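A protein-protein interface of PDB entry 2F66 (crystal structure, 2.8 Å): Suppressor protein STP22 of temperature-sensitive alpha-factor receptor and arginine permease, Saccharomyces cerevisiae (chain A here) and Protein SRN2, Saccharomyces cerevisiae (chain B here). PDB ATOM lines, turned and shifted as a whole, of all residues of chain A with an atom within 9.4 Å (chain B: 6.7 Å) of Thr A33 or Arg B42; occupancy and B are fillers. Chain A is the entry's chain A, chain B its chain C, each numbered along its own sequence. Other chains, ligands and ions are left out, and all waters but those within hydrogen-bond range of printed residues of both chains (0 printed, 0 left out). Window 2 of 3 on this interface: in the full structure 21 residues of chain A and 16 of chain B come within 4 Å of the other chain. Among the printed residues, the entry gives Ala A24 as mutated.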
ATOM      1  N   ALA A  24      -4.664  15.452 -13.878  1.00  0.00           N
ATOM      2  CA  ALA A  24      -4.867  16.579 -14.780  1.00  0.00           C
ATOM      3  C   ALA A  24      -6.227  16.470 -15.450  1.00  0.00           C
ATOM      4  O   ALA A  24      -6.959  17.457 -15.554  1.00  0.00           O
ATOM      5  CB  ALA A  24      -3.768  16.614 -15.838  1.00  0.00           C
ATOM      6  N   LEU A  25      -6.549  15.267 -15.912  1.00  0.00           N
ATOM      7  CA  LEU A  25      -7.818  15.010 -16.556  1.00  0.00           C
ATOM      8  C   LEU A  25      -8.959  15.300 -15.581  1.00  0.00           C
ATOM      9  O   LEU A  25     -10.026  15.760 -15.983  1.00  0.00           O
ATOM     10  CB  LEU A  25      -7.856  13.561 -17.026  1.00  0.00           C
ATOM     11  CG  LEU A  25      -7.759  13.349 -18.541  1.00  0.00           C
ATOM     12  CD1 LEU A  25      -6.937  14.459 -19.183  1.00  0.00           C
ATOM     13  CD2 LEU A  25      -7.163  11.976 -18.832  1.00  0.00           C
ATOM     14  N   SER A  26      -8.720  15.046 -14.295  1.00  0.00           N
ATOM     15  CA  SER A  26      -9.717  15.297 -13.255  1.00  0.00           C
ATOM     16  C   SER A  26     -10.038  16.776 -13.181  1.00  0.00           C
ATOM     17  O   SER A  26     -11.203  17.159 -13.073  1.00  0.00           O
ATOM     18  CB  SER A  26      -9.204  14.849 -11.885  1.00  0.00           C
ATOM     19  OG  SER A  26      -9.187  13.440 -11.780  1.00  0.00           O
ATOM     20  N   ARG A  27      -8.992  17.600 -13.216  1.00  0.00           N
ATOM     21  CA  ARG A  27      -9.157  19.047 -13.155  1.00  0.00           C
ATOM     22  C   ARG A  27      -9.900  19.534 -14.382  1.00  0.00           C
ATOM     23  O   ARG A  27     -10.707  20.448 -14.303  1.00  0.00           O
ATOM     24  CB  ARG A  27      -7.802  19.743 -13.079  1.00  0.00           C
ATOM     25  CG  ARG A  27      -6.977  19.384 -11.859  1.00  0.00           C
ATOM     26  CD  ARG A  27      -5.557  19.935 -11.980  1.00  0.00           C
ATOM     27  NE  ARG A  27      -4.621  19.050 -11.306  1.00  0.00           N
ATOM     28  CZ  ARG A  27      -3.486  18.606 -11.832  1.00  0.00           C
ATOM     29  NH1 ARG A  27      -3.116  18.966 -13.057  1.00  0.00           N
ATOM     30  NH2 ARG A  27      -2.728  17.772 -11.133  1.00  0.00           N
ATOM     31  N   MET A  28      -9.621  18.929 -15.525  1.00  0.00           N
ATOM     32  CA  MET A  28     -10.304  19.328 -16.742  1.00  0.00           C
ATOM     33  C   MET A  28     -11.789  18.990 -16.633  1.00  0.00           C
ATOM     34  O   MET A  28     -12.631  19.689 -17.200  1.00  0.00           O
ATOM     35  CB  MET A  28      -9.659  18.643 -17.946  1.00  0.00           C
ATOM     36  CG  MET A  28      -8.240  19.130 -18.175  1.00  0.00           C
ATOM     37  SD  MET A  28      -7.379  18.275 -19.495  1.00  0.00           S
ATOM     38  CE  MET A  28      -8.428  18.626 -20.866  1.00  0.00           C
ATOM     39  N   LEU A  29     -12.110  17.926 -15.900  1.00  0.00           N
ATOM     40  CA  LEU A  29     -13.502  17.531 -15.702  1.00  0.00           C
ATOM     41  C   LEU A  29     -14.161  18.566 -14.797  1.00  0.00           C
ATOM     42  O   LEU A  29     -15.275  19.038 -15.062  1.00  0.00           O
ATOM     43  CB  LEU A  29     -13.596  16.160 -15.025  1.00  0.00           C
ATOM     44  CG  LEU A  29     -15.013  15.743 -14.607  1.00  0.00           C
ATOM     45  CD1 LEU A  29     -15.862  15.486 -15.840  1.00  0.00           C
ATOM     46  CD2 LEU A  29     -14.958  14.498 -13.752  1.00  0.00           C
ATOM     47  N   HIS A  30     -13.457  18.907 -13.723  1.00  0.00           N
ATOM     48  CA  HIS A  30     -13.938  19.874 -12.750  1.00  0.00           C
ATOM     49  C   HIS A  30     -14.160  21.256 -13.358  1.00  0.00           C
ATOM     50  O   HIS A  30     -15.174  21.902 -13.106  1.00  0.00           O
ATOM     51  CB  HIS A  30     -12.944  19.982 -11.600  1.00  0.00           C
ATOM     52  CG  HIS A  30     -13.360  20.947 -10.538  1.00  0.00           C
ATOM     53  ND1 HIS A  30     -14.545  20.822  -9.845  1.00  0.00           N
ATOM     54  CD2 HIS A  30     -12.749  22.051 -10.048  1.00  0.00           C
ATOM     55  CE1 HIS A  30     -14.644  21.808  -8.971  1.00  0.00           C
ATOM     56  NE2 HIS A  30     -13.568  22.566  -9.074  1.00  0.00           N
ATOM     57  N   ARG A  31     -13.203  21.705 -14.158  1.00  0.00           N
ATOM     58  CA  ARG A  31     -13.284  23.009 -14.794  1.00  0.00           C
ATOM     59  C   ARG A  31     -14.284  23.031 -15.936  1.00  0.00           C
ATOM     60  O   ARG A  31     -14.495  24.067 -16.554  1.00  0.00           O
ATOM     61  CB  ARG A  31     -11.903  23.440 -15.309  1.00  0.00           C
ATOM     62  CG  ARG A  31     -10.921  23.813 -14.202  1.00  0.00           C
ATOM     63  CD  ARG A  31      -9.664  24.447 -14.766  1.00  0.00           C
ATOM     64  NE  ARG A  31      -8.727  23.465 -15.308  1.00  0.00           N
ATOM     65  CZ  ARG A  31      -7.806  22.832 -14.586  1.00  0.00           C
ATOM     66  NH1 ARG A  31      -7.691  23.077 -13.285  1.00  0.00           N
ATOM     67  NH2 ARG A  31      -7.001  21.950 -15.166  1.00  0.00           N
ATOM     68  N   GLY A  32     -14.899  21.893 -16.221  1.00  0.00           N
ATOM     69  CA  GLY A  32     -15.865  21.848 -17.304  1.00  0.00           C
ATOM     70  C   GLY A  32     -15.248  21.699 -18.687  1.00  0.00           C
ATOM     71  O   GLY A  32     -15.965  21.663 -19.683  1.00  0.00           O
ATOM     72  N   THR A  33     -13.924  21.599 -18.751  1.00  0.00           N
ATOM     73  CA  THR A  33     -13.218  21.457 -20.019  1.00  0.00           C
ATOM     74  C   THR A  33     -13.614  20.186 -20.771  1.00  0.00           C
ATOM     75  O   THR A  33     -13.751  20.206 -21.993  1.00  0.00           O
ATOM     76  CB  THR A  33     -11.708  21.441 -19.797  1.00  0.00           C
ATOM     77  OG1 THR A  33     -11.351  22.485 -18.886  1.00  0.00           O
ATOM     78  CG2 THR A  33     -10.983  21.668 -21.111  1.00  0.00           C
ATOM     79  N   ILE A  34     -13.782  19.084 -20.035  1.00  0.00           N
ATOM     80  CA  ILE A  34     -14.183  17.790 -20.604  1.00  0.00           C
ATOM     81  C   ILE A  34     -15.308  17.171 -19.783  1.00  0.00           C
ATOM     82  O   ILE A  34     -15.419  17.401 -18.573  1.00  0.00           O
ATOM     83  CB  ILE A  34     -13.020  16.762 -20.629  1.00  0.00           C
ATOM     84  CG1 ILE A  34     -12.437  16.607 -19.222  1.00  0.00           C
ATOM     85  CG2 ILE A  34     -11.954  17.187 -21.622  1.00  0.00           C
ATOM     86  CD1 ILE A  34     -11.280  15.632 -19.115  1.00  0.00           C
ATOM     87  N   PRO A  35     -16.164  16.370 -20.435  1.00  0.00           N
ATOM     88  CA  PRO A  35     -17.290  15.705 -19.772  1.00  0.00           C
ATOM     89  C   PRO A  35     -16.870  14.431 -19.032  1.00  0.00           C
ATOM     90  O   PRO A  35     -15.766  13.916 -19.214  1.00  0.00           O
ATOM     91  CB  PRO A  35     -18.236  15.406 -20.929  1.00  0.00           C
ATOM     92  CG  PRO A  35     -17.285  15.069 -22.030  1.00  0.00           C
ATOM     93  CD  PRO A  35     -16.212  16.150 -21.892  1.00  0.00           C
ATOM     94  N   LEU A  36     -17.776  13.918 -18.216  1.00  0.00           N
ATOM     95  CA  LEU A  36     -17.514  12.719 -17.446  1.00  0.00           C
ATOM     96  C   LEU A  36     -17.116  11.526 -18.306  1.00  0.00           C
ATOM     97  O   LEU A  36     -16.090  10.884 -18.051  1.00  0.00           O
ATOM     98  CB  LEU A  36     -18.749  12.353 -16.613  1.00  0.00           C
ATOM     99  CG  LEU A  36     -18.671  11.125 -15.694  1.00  0.00           C
ATOM    100  CD1 LEU A  36     -17.442  11.202 -14.770  1.00  0.00           C
ATOM    101  CD2 LEU A  36     -19.952  11.048 -14.877  1.00  0.00           C
ATOM    102  N   THR A  38     -15.770  11.305 -21.091  1.00  0.00           N
ATOM    103  CA  THR A  38     -14.449  11.426 -21.679  1.00  0.00           C
ATOM    104  C   THR A  38     -13.405  11.073 -20.633  1.00  0.00           C
ATOM    105  O   THR A  38     -12.481  10.306 -20.897  1.00  0.00           O
ATOM    106  CB  THR A  38     -14.217  12.836 -22.209  1.00  0.00           C
ATOM    107  OG1 THR A  38     -15.129  13.076 -23.283  1.00  0.00           O
ATOM    108  CG2 THR A  38     -12.803  12.989 -22.732  1.00  0.00           C
ATOM    109  N   PHE A  39     -13.564  11.619 -19.437  1.00  0.00           N
ATOM    110  CA  PHE A  39     -12.642  11.326 -18.355  1.00  0.00           C
ATOM    111  C   PHE A  39     -12.574   9.822 -18.094  1.00  0.00           C
ATOM    112  O   PHE A  39     -11.502   9.242 -17.977  1.00  0.00           O
ATOM    113  CB  PHE A  39     -13.083  12.009 -17.068  1.00  0.00           C
ATOM    114  CG  PHE A  39     -12.209  11.676 -15.906  1.00  0.00           C
ATOM    115  CD1 PHE A  39     -10.920  12.202 -15.820  1.00  0.00           C
ATOM    116  CD2 PHE A  39     -12.641  10.787 -14.929  1.00  0.00           C
ATOM    117  CE1 PHE A  39     -10.070  11.843 -14.775  1.00  0.00           C
ATOM    118  CE2 PHE A  39     -11.803  10.421 -13.882  1.00  0.00           C
ATOM    119  CZ  PHE A  39     -10.511  10.951 -13.805  1.00  0.00           C
ATOM    120  N   LEU B  37       1.098  23.997 -20.117  1.00  0.00           N
ATOM    121  CA  LEU B  37       0.299  23.271 -21.097  1.00  0.00           C
ATOM    122  C   LEU B  37      -1.126  23.089 -20.598  1.00  0.00           C
ATOM    123  O   LEU B  37      -2.091  23.242 -21.351  1.00  0.00           O
ATOM    124  CB  LEU B  37       0.919  21.898 -21.370  1.00  0.00           C
ATOM    125  CG  LEU B  37       0.133  21.014 -22.342  1.00  0.00           C
ATOM    126  CD1 LEU B  37      -0.074  21.755 -23.646  1.00  0.00           C
ATOM    127  CD2 LEU B  37       0.872  19.714 -22.584  1.00  0.00           C
ATOM    128  N   GLU B  38      -1.252  22.768 -19.317  1.00  0.00           N
ATOM    129  CA  GLU B  38      -2.558  22.552 -18.728  1.00  0.00           C
ATOM    130  C   GLU B  38      -3.396  23.813 -18.786  1.00  0.00           C
ATOM    131  O   GLU B  38      -4.568  23.765 -19.163  1.00  0.00           O
ATOM    132  CB  GLU B  38      -2.413  22.071 -17.283  1.00  0.00           C
ATOM    133  CG  GLU B  38      -3.736  21.790 -16.596  1.00  0.00           C
ATOM    134  CD  GLU B  38      -3.571  21.038 -15.292  1.00  0.00           C
ATOM    135  OE1 GLU B  38      -2.432  20.964 -14.782  1.00  0.00           O
ATOM    136  OE2 GLU B  38      -4.585  20.527 -14.773  1.00  0.00           O
ATOM    137  N   THR B  39      -2.798  24.941 -18.416  1.00  0.00           N
ATOM    138  CA  THR B  39      -3.505  26.219 -18.445  1.00  0.00           C
ATOM    139  C   THR B  39      -3.921  26.580 -19.863  1.00  0.00           C
ATOM    140  O   THR B  39      -5.038  27.024 -20.101  1.00  0.00           O
ATOM    141  CB  THR B  39      -2.631  27.346 -17.902  1.00  0.00           C
ATOM    142  OG1 THR B  39      -2.632  27.296 -16.470  1.00  0.00           O
ATOM    143  CG2 THR B  39      -3.150  28.688 -18.370  1.00  0.00           C
ATOM    144  N   THR B  40      -2.998  26.387 -20.795  1.00  0.00           N
ATOM    145  CA  THR B  40      -3.229  26.662 -22.202  1.00  0.00           C
ATOM    146  C   THR B  40      -4.397  25.848 -22.746  1.00  0.00           C
ATOM    147  O   THR B  40      -5.240  26.364 -23.477  1.00  0.00           O
ATOM    148  CB  THR B  40      -1.966  26.329 -23.022  1.00  0.00           C
ATOM    149  OG1 THR B  40      -0.926  27.253 -22.676  1.00  0.00           O
ATOM    150  CG2 THR B  40      -2.251  26.393 -24.526  1.00  0.00           C
ATOM    151  N   THR B  41      -4.442  24.570 -22.394  1.00  0.00           N
ATOM    152  CA  THR B  41      -5.508  23.698 -22.869  1.00  0.00           C
ATOM    153  C   THR B  41      -6.822  24.020 -22.165  1.00  0.00           C
ATOM    154  O   THR B  41      -7.284  23.266 -21.305  1.00  0.00           O
ATOM    155  CB  THR B  41      -5.157  22.230 -22.620  1.00  0.00           C
ATOM    156  OG1 THR B  41      -3.857  21.959 -23.159  1.00  0.00           O
ATOM    157  CG2 THR B  41      -6.182  21.320 -23.286  1.00  0.00           C
ATOM    158  N   ARG B  42      -7.430  25.137 -22.545  1.00  0.00           N
ATOM    159  CA  ARG B  42      -8.671  25.553 -21.920  1.00  0.00           C
ATOM    160  C   ARG B  42      -9.900  25.082 -22.679  1.00  0.00           C
ATOM    161  O   ARG B  42     -11.023  25.438 -22.337  1.00  0.00           O
ATOM    162  CB  ARG B  42      -8.689  27.074 -21.769  1.00  0.00           C
ATOM    163  CG  ARG B  42      -9.760  27.573 -20.821  1.00  0.00           C
ATOM    164  CD  ARG B  42      -9.679  29.073 -20.627  1.00  0.00           C
ATOM    165  NE  ARG B  42     -10.764  29.568 -19.785  1.00  0.00           N
ATOM    166  CZ  ARG B  42     -10.968  30.854 -19.509  1.00  0.00           C
ATOM    167  NH1 ARG B  42     -10.156  31.778 -20.007  1.00  0.00           N
ATOM    168  NH2 ARG B  42     -11.987  31.217 -18.740  1.00  0.00           N
ATOM    169  N   SER B  43      -9.690  24.267 -23.703  1.00  0.00           N
ATOM    170  CA  SER B  43     -10.808  23.753 -24.479  1.00  0.00           C
ATOM    171  C   SER B  43     -10.405  22.634 -25.424  1.00  0.00           C
ATOM    172  O   SER B  43      -9.400  22.729 -26.129  1.00  0.00           O
ATOM    173  CB  SER B  43     -11.459  24.886 -25.269  1.00  0.00           C
ATOM    174  OG  SER B  43     -10.477  25.638 -25.952  1.00  0.00           O
ATOM    175  N   ILE B  44     -11.191  21.562 -25.417  1.00  0.00           N
ATOM    176  CA  ILE B  44     -10.949  20.413 -26.286  1.00  0.00           C
ATOM    177  C   ILE B  44     -12.169  20.277 -27.195  1.00  0.00           C
ATOM    178  O   ILE B  44     -13.294  20.107 -26.720  1.00  0.00           O
ATOM    179  CB  ILE B  44     -10.751  19.094 -25.473  1.00  0.00           C
ATOM    180  CG1 ILE B  44      -9.395  19.106 -24.753  1.00  0.00           C
ATOM    181  CG2 ILE B  44     -10.807  17.890 -26.407  1.00  0.00           C
ATOM    182  CD1 ILE B  44      -9.283  20.127 -23.654  1.00  0.00           C
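OE1 of Glu B38 lies within salt-bridge range of NH1 of Arg A27 (2.7 Å). OE2 of Glu B38 is in salt-bridge range of NH2 of Arg A31, 2.8 Å away.
Hydrophobic or aromatic side chains of chain B that line the printed part of chain A: Ile B44. Printed residues of chain A that touch a printed residue of chain B: Ala A24, Arg A27, Met A28, Arg A31 and Thr A33. Hydrophobic or aromatic side chains of chain A within 4 Å of the printed part of chain B: Met A28. Among the printed residues, Asp or Glu carboxylates within 4 Å of a Lys or Arg side-chain nitrogen of the other chain: Arg A27 with Glu B38 (2.7 Å) and Arg A31 with Glu B38 (2.8 Å).
Thr A33 touches just these residues of chain B: Arg B42, Ser B43 and Ile B44. Arg B42 touches just one residue of chain A: Thr A33 (3.9 Å). No residue of chain A comes within 4 Å of Thr B41. Ser B43 touches just one residue of chain A: Thr A33 (3.9 Å). Printed residues of chain A within 4 Å of Glu B38: Ala A24 (3.96 Å), Arg A27 (2.7 Å) and Arg A31 (2.8 Å). Of the printed residues of chain B, Ala A24 touches Glu B38 (3.96 Å). Of the printed residues of chain B, Arg A31 touches Glu B38. Of the printed residues of chain A, Ile B44 touches Met A28 (3.3 Å) and Thr A33 (3.4 Å). Phe A39 touches none of the printed residues of chain B. The nearest printed residue of chain B that does not touch Ala A24 is Thr B41 (8.2 Å).
OE2 of Glu B38 touches CA of Ala A24, at 3.96 Å. Met A28 touches Ile B44. Thr A33 touches Arg B42 (CG2 to C, 3.9 Å). CG2 of Thr A33 touches N of Ser B43, at 3.9 Å. Ile B44 touches Thr A33 (CD1 to CG2, 3.4 Å).
The backbone carbonyl oxygen of Met A28 lies within hydrogen-bond range of the backbone NH of Thr A33, 2.8 Å away. O of Met A28 sits at hydrogen-bond distance from N of Ile A34.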
